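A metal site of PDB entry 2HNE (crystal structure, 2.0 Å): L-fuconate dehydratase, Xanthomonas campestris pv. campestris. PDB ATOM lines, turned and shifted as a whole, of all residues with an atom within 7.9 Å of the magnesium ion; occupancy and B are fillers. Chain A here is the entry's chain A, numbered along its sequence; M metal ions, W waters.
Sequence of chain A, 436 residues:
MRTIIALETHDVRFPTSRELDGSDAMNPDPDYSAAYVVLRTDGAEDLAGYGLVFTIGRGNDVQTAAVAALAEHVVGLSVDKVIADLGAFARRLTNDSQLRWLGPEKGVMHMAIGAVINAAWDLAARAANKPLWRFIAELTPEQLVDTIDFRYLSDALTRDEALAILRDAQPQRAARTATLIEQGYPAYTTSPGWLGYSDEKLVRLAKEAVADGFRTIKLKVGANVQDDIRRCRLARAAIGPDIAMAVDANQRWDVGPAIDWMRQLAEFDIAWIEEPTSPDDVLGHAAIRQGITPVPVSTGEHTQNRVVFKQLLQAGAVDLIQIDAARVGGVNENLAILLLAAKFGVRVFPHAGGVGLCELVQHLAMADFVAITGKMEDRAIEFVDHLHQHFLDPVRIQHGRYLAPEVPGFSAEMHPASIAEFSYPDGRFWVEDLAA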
ATOM      1  N   TYR A 188      12.291  22.926 -23.138  1.00  0.00           N
ATOM      2  CA  TYR A 188      13.030  24.079 -22.639  1.00  0.00           C
ATOM      3  C   TYR A 188      14.388  24.053 -23.329  1.00  0.00           C
ATOM      4  O   TYR A 188      14.825  23.004 -23.769  1.00  0.00           O
ATOM      5  CB  TYR A 188      13.197  24.065 -21.106  1.00  0.00           C
ATOM      6  CG  TYR A 188      14.053  22.962 -20.514  1.00  0.00           C
ATOM      7  CD1 TYR A 188      13.543  21.676 -20.349  1.00  0.00           C
ATOM      8  CD2 TYR A 188      15.327  23.236 -20.033  1.00  0.00           C
ATOM      9  CE1 TYR A 188      14.291  20.672 -19.719  1.00  0.00           C
ATOM     10  CE2 TYR A 188      16.095  22.241 -19.398  1.00  0.00           C
ATOM     11  CZ  TYR A 188      15.567  20.965 -19.240  1.00  0.00           C
ATOM     12  OH  TYR A 188      16.300  19.972 -18.626  1.00  0.00           O
ATOM     13  N   THR A 190      18.640  25.169 -23.583  1.00  0.00           N
ATOM     14  CA  THR A 190      19.871  25.484 -22.878  1.00  0.00           C
ATOM     15  C   THR A 190      20.832  26.185 -23.845  1.00  0.00           C
ATOM     16  O   THR A 190      21.887  26.669 -23.447  1.00  0.00           O
ATOM     17  CB  THR A 190      20.524  24.206 -22.359  1.00  0.00           C
ATOM     18  OG1 THR A 190      20.737  23.302 -23.443  1.00  0.00           O
ATOM     19  CG2 THR A 190      19.613  23.535 -21.341  1.00  0.00           C
ATOM     20  N   LYS A 218      17.578  27.805 -19.684  1.00  0.00           N
ATOM     21  CA  LYS A 218      18.541  27.443 -18.637  1.00  0.00           C
ATOM     22  C   LYS A 218      19.943  27.936 -19.004  1.00  0.00           C
ATOM     23  O   LYS A 218      20.413  27.728 -20.110  1.00  0.00           O
ATOM     24  CB  LYS A 218      18.581  25.932 -18.417  1.00  0.00           C
ATOM     25  CG  LYS A 218      19.366  25.523 -17.172  1.00  0.00           C
ATOM     26  CD  LYS A 218      19.224  24.035 -16.861  1.00  0.00           C
ATOM     27  CE  LYS A 218      19.936  23.178 -17.882  1.00  0.00           C
ATOM     28  NZ  LYS A 218      19.647  21.738 -17.662  1.00  0.00           N
ATOM     29  N   LYS A 220      24.174  28.375 -17.784  1.00  0.00           N
ATOM     30  CA  LYS A 220      25.234  27.757 -16.997  1.00  0.00           C
ATOM     31  C   LYS A 220      25.811  28.825 -16.090  1.00  0.00           C
ATOM     32  O   LYS A 220      25.854  30.017 -16.437  1.00  0.00           O
ATOM     33  CB  LYS A 220      26.338  27.220 -17.902  1.00  0.00           C
ATOM     34  CG  LYS A 220      25.895  26.097 -18.783  1.00  0.00           C
ATOM     35  CD  LYS A 220      27.055  25.417 -19.462  1.00  0.00           C
ATOM     36  CE  LYS A 220      26.541  24.285 -20.320  1.00  0.00           C
ATOM     37  NZ  LYS A 220      25.549  23.462 -19.564  1.00  0.00           N
ATOM     38  N   VAL A 247      19.168  27.575 -13.883  1.00  0.00           N
ATOM     39  CA  VAL A 247      20.625  27.667 -13.889  1.00  0.00           C
ATOM     40  C   VAL A 247      21.246  26.279 -13.647  1.00  0.00           C
ATOM     41  O   VAL A 247      20.666  25.449 -12.940  1.00  0.00           O
ATOM     42  CB  VAL A 247      21.067  28.662 -12.799  1.00  0.00           C
ATOM     43  CG1 VAL A 247      22.432  28.326 -12.315  1.00  0.00           C
ATOM     44  CG2 VAL A 247      21.026  30.094 -13.355  1.00  0.00           C
ATOM     45  N   ASP A 248      22.410  26.044 -14.244  1.00  0.00           N
ATOM     46  CA  ASP A 248      23.096  24.746 -14.123  1.00  0.00           C
ATOM     47  C   ASP A 248      24.556  24.940 -13.692  1.00  0.00           C
ATOM     48  O   ASP A 248      25.359  25.527 -14.413  1.00  0.00           O
ATOM     49  CB  ASP A 248      23.058  24.054 -15.490  1.00  0.00           C
ATOM     50  CG  ASP A 248      23.364  22.584 -15.410  1.00  0.00           C
ATOM     51  OD1 ASP A 248      24.144  22.153 -14.542  1.00  0.00           O
ATOM     52  OD2 ASP A 248      22.831  21.851 -16.261  1.00  0.00           O
ATOM     53  N   ALA A 249      24.898  24.427 -12.506  1.00  0.00           N
ATOM     54  CA  ALA A 249      26.275  24.549 -11.994  1.00  0.00           C
ATOM     55  C   ALA A 249      27.134  23.345 -12.352  1.00  0.00           C
ATOM     56  O   ALA A 249      28.345  23.326 -12.097  1.00  0.00           O
ATOM     57  CB  ALA A 249      26.247  24.739 -10.485  1.00  0.00           C
ATOM     58  N   ASN A 250      26.514  22.348 -12.956  1.00  0.00           N
ATOM     59  CA  ASN A 250      27.233  21.146 -13.366  1.00  0.00           C
ATOM     60  C   ASN A 250      28.165  20.522 -12.331  1.00  0.00           C
ATOM     61  O   ASN A 250      29.328  20.231 -12.626  1.00  0.00           O
ATOM     62  CB  ASN A 250      28.009  21.427 -14.648  1.00  0.00           C
ATOM     63  CG  ASN A 250      27.108  21.560 -15.863  1.00  0.00           C
ATOM     64  OD1 ASN A 250      26.670  20.562 -16.446  1.00  0.00           O
ATOM     65  ND2 ASN A 250      26.806  22.802 -16.233  1.00  0.00           N
ATOM     66  N   GLN A 251      27.665  20.342 -11.101  1.00  0.00           N
ATOM     67  CA  GLN A 251      28.417  19.673 -10.037  1.00  0.00           C
ATOM     68  C   GLN A 251      29.660  20.393  -9.496  1.00  0.00           C
ATOM     69  O   GLN A 251      30.438  19.796  -8.740  1.00  0.00           O
ATOM     70  CB  GLN A 251      28.838  18.285 -10.525  1.00  0.00           C
ATOM     71  CG  GLN A 251      27.723  17.444 -11.180  1.00  0.00           C
ATOM     72  CD  GLN A 251      28.273  16.189 -11.882  1.00  0.00           C
ATOM     73  OE1 GLN A 251      29.463  15.897 -11.812  1.00  0.00           O
ATOM     74  NE2 GLN A 251      27.395  15.437 -12.566  1.00  0.00           N
ATOM     75  N   TRP A 272      15.276  27.063 -11.020  1.00  0.00           N
ATOM     76  CA  TRP A 272      15.913  25.999 -10.245  1.00  0.00           C
ATOM     77  C   TRP A 272      17.404  26.003 -10.533  1.00  0.00           C
ATOM     78  O   TRP A 272      17.828  26.476 -11.597  1.00  0.00           O
ATOM     79  CB  TRP A 272      15.309  24.616 -10.565  1.00  0.00           C
ATOM     80  CG  TRP A 272      15.760  23.972 -11.872  1.00  0.00           C
ATOM     81  CD1 TRP A 272      16.919  23.284 -12.098  1.00  0.00           C
ATOM     82  CD2 TRP A 272      15.029  23.949 -13.109  1.00  0.00           C
ATOM     83  NE1 TRP A 272      16.952  22.814 -13.394  1.00  0.00           N
ATOM     84  CE2 TRP A 272      15.797  23.207 -14.037  1.00  0.00           C
ATOM     85  CE3 TRP A 272      13.785  24.471 -13.524  1.00  0.00           C
ATOM     86  CZ2 TRP A 272      15.375  22.974 -15.353  1.00  0.00           C
ATOM     87  CZ3 TRP A 272      13.373  24.237 -14.837  1.00  0.00           C
ATOM     88  CH2 TRP A 272      14.162  23.497 -15.728  1.00  0.00           C
ATOM     89  N   GLU A 274      20.416  23.510 -11.045  1.00  0.00           N
ATOM     90  CA  GLU A 274      20.658  22.117 -11.426  1.00  0.00           C
ATOM     91  C   GLU A 274      22.065  21.683 -11.040  1.00  0.00           C
ATOM     92  O   GLU A 274      23.036  22.413 -11.230  1.00  0.00           O
ATOM     93  CB  GLU A 274      20.459  21.976 -12.933  1.00  0.00           C
ATOM     94  CG  GLU A 274      20.602  20.566 -13.477  1.00  0.00           C
ATOM     95  CD  GLU A 274      19.947  20.419 -14.830  1.00  0.00           C
ATOM     96  OE1 GLU A 274      18.862  21.008 -15.021  1.00  0.00           O
ATOM     97  OE2 GLU A 274      20.493  19.722 -15.703  1.00  0.00           O
ATOM     98  N   GLU A 275      22.155  20.480 -10.474  1.00  0.00           N
ATOM     99  CA  GLU A 275      23.414  19.900 -10.024  1.00  0.00           C
ATOM    100  C   GLU A 275      24.359  20.841  -9.297  1.00  0.00           C
ATOM    101  O   GLU A 275      25.490  21.036  -9.728  1.00  0.00           O
ATOM    102  CB  GLU A 275      24.172  19.283 -11.196  1.00  0.00           C
ATOM    103  CG  GLU A 275      23.432  18.168 -11.890  1.00  0.00           C
ATOM    104  CD  GLU A 275      24.390  17.159 -12.481  1.00  0.00           C
ATOM    105  OE1 GLU A 275      24.754  16.180 -11.786  1.00  0.00           O
ATOM    106  OE2 GLU A 275      24.791  17.347 -13.657  1.00  0.00           O
ATOM    107  N   SER A 298      17.583  20.847  -8.193  1.00  0.00           N
ATOM    108  CA  SER A 298      17.357  19.636  -8.988  1.00  0.00           C
ATOM    109  C   SER A 298      18.683  18.934  -9.247  1.00  0.00           C
ATOM    110  O   SER A 298      19.761  19.494  -9.044  1.00  0.00           O
ATOM    111  CB  SER A 298      16.715  19.963 -10.347  1.00  0.00           C
ATOM    112  OG  SER A 298      17.709  20.036 -11.366  1.00  0.00           O
ATOM    113  N   THR A 299      18.568  17.690  -9.690  1.00  0.00           N
ATOM    114  CA  THR A 299      19.701  16.848 -10.046  1.00  0.00           C
ATOM    115  C   THR A 299      19.071  15.647 -10.749  1.00  0.00           C
ATOM    116  O   THR A 299      17.835  15.506 -10.756  1.00  0.00           O
ATOM    117  CB  THR A 299      20.501  16.366  -8.808  1.00  0.00           C
ATOM    118  OG1 THR A 299      21.703  15.710  -9.236  1.00  0.00           O
ATOM    119  CG2 THR A 299      19.682  15.356  -7.985  1.00  0.00           C
ATOM    120  N   GLY A 300      19.900  14.805 -11.350  1.00  0.00           N
ATOM    121  CA  GLY A 300      19.357  13.621 -11.988  1.00  0.00           C
ATOM    122  C   GLY A 300      19.988  13.110 -13.264  1.00  0.00           C
ATOM    123  O   GLY A 300      19.915  11.920 -13.545  1.00  0.00           O
ATOM    124  N   GLU A 301      20.619  13.984 -14.057  1.00  0.00           N
ATOM    125  CA  GLU A 301      21.195  13.512 -15.313  1.00  0.00           C
ATOM    126  C   GLU A 301      22.339  12.531 -15.119  1.00  0.00           C
ATOM    127  O   GLU A 301      22.643  11.749 -16.017  1.00  0.00           O
ATOM    128  CB  GLU A 301      21.653  14.694 -16.171  1.00  0.00           C
ATOM    129  CG  GLU A 301      22.969  15.319 -15.763  1.00  0.00           C
ATOM    130  CD  GLU A 301      23.217  16.610 -16.519  1.00  0.00           C
ATOM    131  OE1 GLU A 301      22.329  17.480 -16.444  1.00  0.00           O
ATOM    132  OE2 GLU A 301      24.275  16.757 -17.174  1.00  0.00           O
ATOM    133  N   HIS A 302      22.964  12.569 -13.947  1.00  0.00           N
ATOM    134  CA  HIS A 302      24.081  11.676 -13.638  1.00  0.00           C
ATOM    135  C   HIS A 302      23.784  10.732 -12.475  1.00  0.00           C
ATOM    136  O   HIS A 302      24.658   9.984 -12.048  1.00  0.00           O
ATOM    137  CB  HIS A 302      25.330  12.493 -13.299  1.00  0.00           C
ATOM    138  CG  HIS A 302      26.277  12.647 -14.449  1.00  0.00           C
ATOM    139  ND1 HIS A 302      25.866  12.555 -15.762  1.00  0.00           N
ATOM    140  CD2 HIS A 302      27.609  12.904 -14.485  1.00  0.00           C
ATOM    141  CE1 HIS A 302      26.908  12.749 -16.555  1.00  0.00           C
ATOM    142  NE2 HIS A 302      27.971  12.968 -15.810  1.00  0.00           N
ATOM    143  N   GLN A 322      15.823  15.503 -12.920  1.00  0.00           N
ATOM    144  CA  GLN A 322      16.061  15.219 -14.322  1.00  0.00           C
ATOM    145  C   GLN A 322      16.086  13.699 -14.368  1.00  0.00           C
ATOM    146  O   GLN A 322      16.252  13.038 -13.336  1.00  0.00           O
ATOM    147  CB  GLN A 322      17.455  15.693 -14.773  1.00  0.00           C
ATOM    148  CG  GLN A 322      17.560  17.125 -15.255  1.00  0.00           C
ATOM    149  CD  GLN A 322      17.400  18.126 -14.150  1.00  0.00           C
ATOM    150  OE1 GLN A 322      18.115  18.103 -13.152  1.00  0.00           O
ATOM    151  NE2 GLN A 322      16.453  19.036 -14.318  1.00  0.00           N
ATOM    152  N   HIS A 351      16.439  15.271 -19.122  1.00  0.00           N
ATOM    153  CA  HIS A 351      17.706  15.789 -19.594  1.00  0.00           C
ATOM    154  C   HIS A 351      17.837  15.234 -20.996  1.00  0.00           C
ATOM    155  O   HIS A 351      17.381  14.122 -21.273  1.00  0.00           O
ATOM    156  CB  HIS A 351      18.851  15.263 -18.712  1.00  0.00           C
ATOM    157  CG  HIS A 351      20.202  15.367 -19.340  1.00  0.00           C
ATOM    158  ND1 HIS A 351      20.949  16.524 -19.322  1.00  0.00           N
ATOM    159  CD2 HIS A 351      20.948  14.446 -20.005  1.00  0.00           C
ATOM    160  CE1 HIS A 351      22.095  16.319 -19.951  1.00  0.00           C
ATOM    161  NE2 HIS A 351      22.119  15.059 -20.372  1.00  0.00           N
ATOM    162  N   ALA A 352      18.457  15.996 -21.891  1.00  0.00           N
ATOM    163  CA  ALA A 352      18.645  15.530 -23.249  1.00  0.00           C
ATOM    164  C   ALA A 352      19.932  16.082 -23.847  1.00  0.00           C
ATOM    165  O   ALA A 352      20.893  16.372 -23.121  1.00  0.00           O
ATOM    166  CB  ALA A 352      17.453  15.932 -24.115  1.00  0.00           C
ATOM    167  N   GLU A 382      14.184  18.709 -22.142  1.00  0.00           N
ATOM    168  CA  GLU A 382      15.255  19.528 -22.675  1.00  0.00           C
ATOM    169  C   GLU A 382      15.394  19.357 -24.165  1.00  0.00           C
ATOM    170  O   GLU A 382      15.204  18.264 -24.694  1.00  0.00           O
ATOM    171  CB  GLU A 382      16.580  19.180 -21.989  1.00  0.00           C
ATOM    172  CG  GLU A 382      17.783  19.881 -22.613  1.00  0.00           C
ATOM    173  CD  GLU A 382      19.052  19.665 -21.806  1.00  0.00           C
ATOM    174  OE1 GLU A 382      19.368  18.496 -21.496  1.00  0.00           O
ATOM    175  OE2 GLU A 382      19.730  20.661 -21.501  1.00  0.00           O
HETATM  176 MG    MG M   1      22.570  19.655 -16.496  1.00  0.00          MG
HETATM  177  O   HOH W   1      23.825  19.596 -14.623  1.00  0.00           O
HETATM  178  O   HOH W   2      21.351  19.697 -18.565  1.00  0.00           O
HETATM  179  O   HOH W   3      24.558  19.585 -17.765  1.00  0.00           O
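ND1 of His 351 sits close to OE1 of Glu 301 (3.3 Å). The side-chain carboxylate of Glu 274 is in salt-bridge range of the side-chain amino group of Lys 218. The side-chain carboxylate (OE1) of Glu 274 is in hydrogen-bond range of the side-chain amide nitrogen (NE2) of Gln 322, 3.2 Å away. O of Glu 274 lies within hydrogen-bond range of N of Ala 249, at 3.0 Å. The backbone carbonyl oxygen of Val 247 is in hydrogen-bond range of the backbone NH of Glu 274 (2.7 Å). The side-chain carboxylate of Asp 248 sits close to the side-chain amino group of Lys 218 (3.5 Å). OD1 of Asp 248 lies within hydrogen-bond range of N of Asn 250 (2.9 Å). The side-chain amino group (NZ) of Lys 218 is in salt-bridge range of the side-chain carboxylate (OE2) of Glu 382 (3.99 Å).
Residues that only touch the magnesium ion: Lys 218 (3.8 Å). Of the 21 residues printed, 4 come within 4 Å of the magnesium ion.
The magnesium ion is bound by the side-chain carboxylate of Glu 301 (2.2 Å), the side-chain carboxylate of Glu 274 (2.2 Å), the side-chain carboxylate of Asp 248 (2.2 Å), water W1 (2.3 Å), water W3 (2.4 Å) and water W2 (2.4 Å). The magnesium ion has six donor atoms within binding distance.
Water W1 bridges the side-chain carboxylate of Asp 248 (2.6 Å) and the side-chain carboxylate of Glu 275 (2.6 Å). Water W3 bridges the side-chain amide oxygen (OD1) of Asn 250 (2.7 Å) and the side-chain carboxylate (OE2) of Glu 301 (2.9 Å). Water W2 lies within hydrogen-bond range of NZ of Lys 218, ND1 of His 351 and OE2 of Glu 382.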
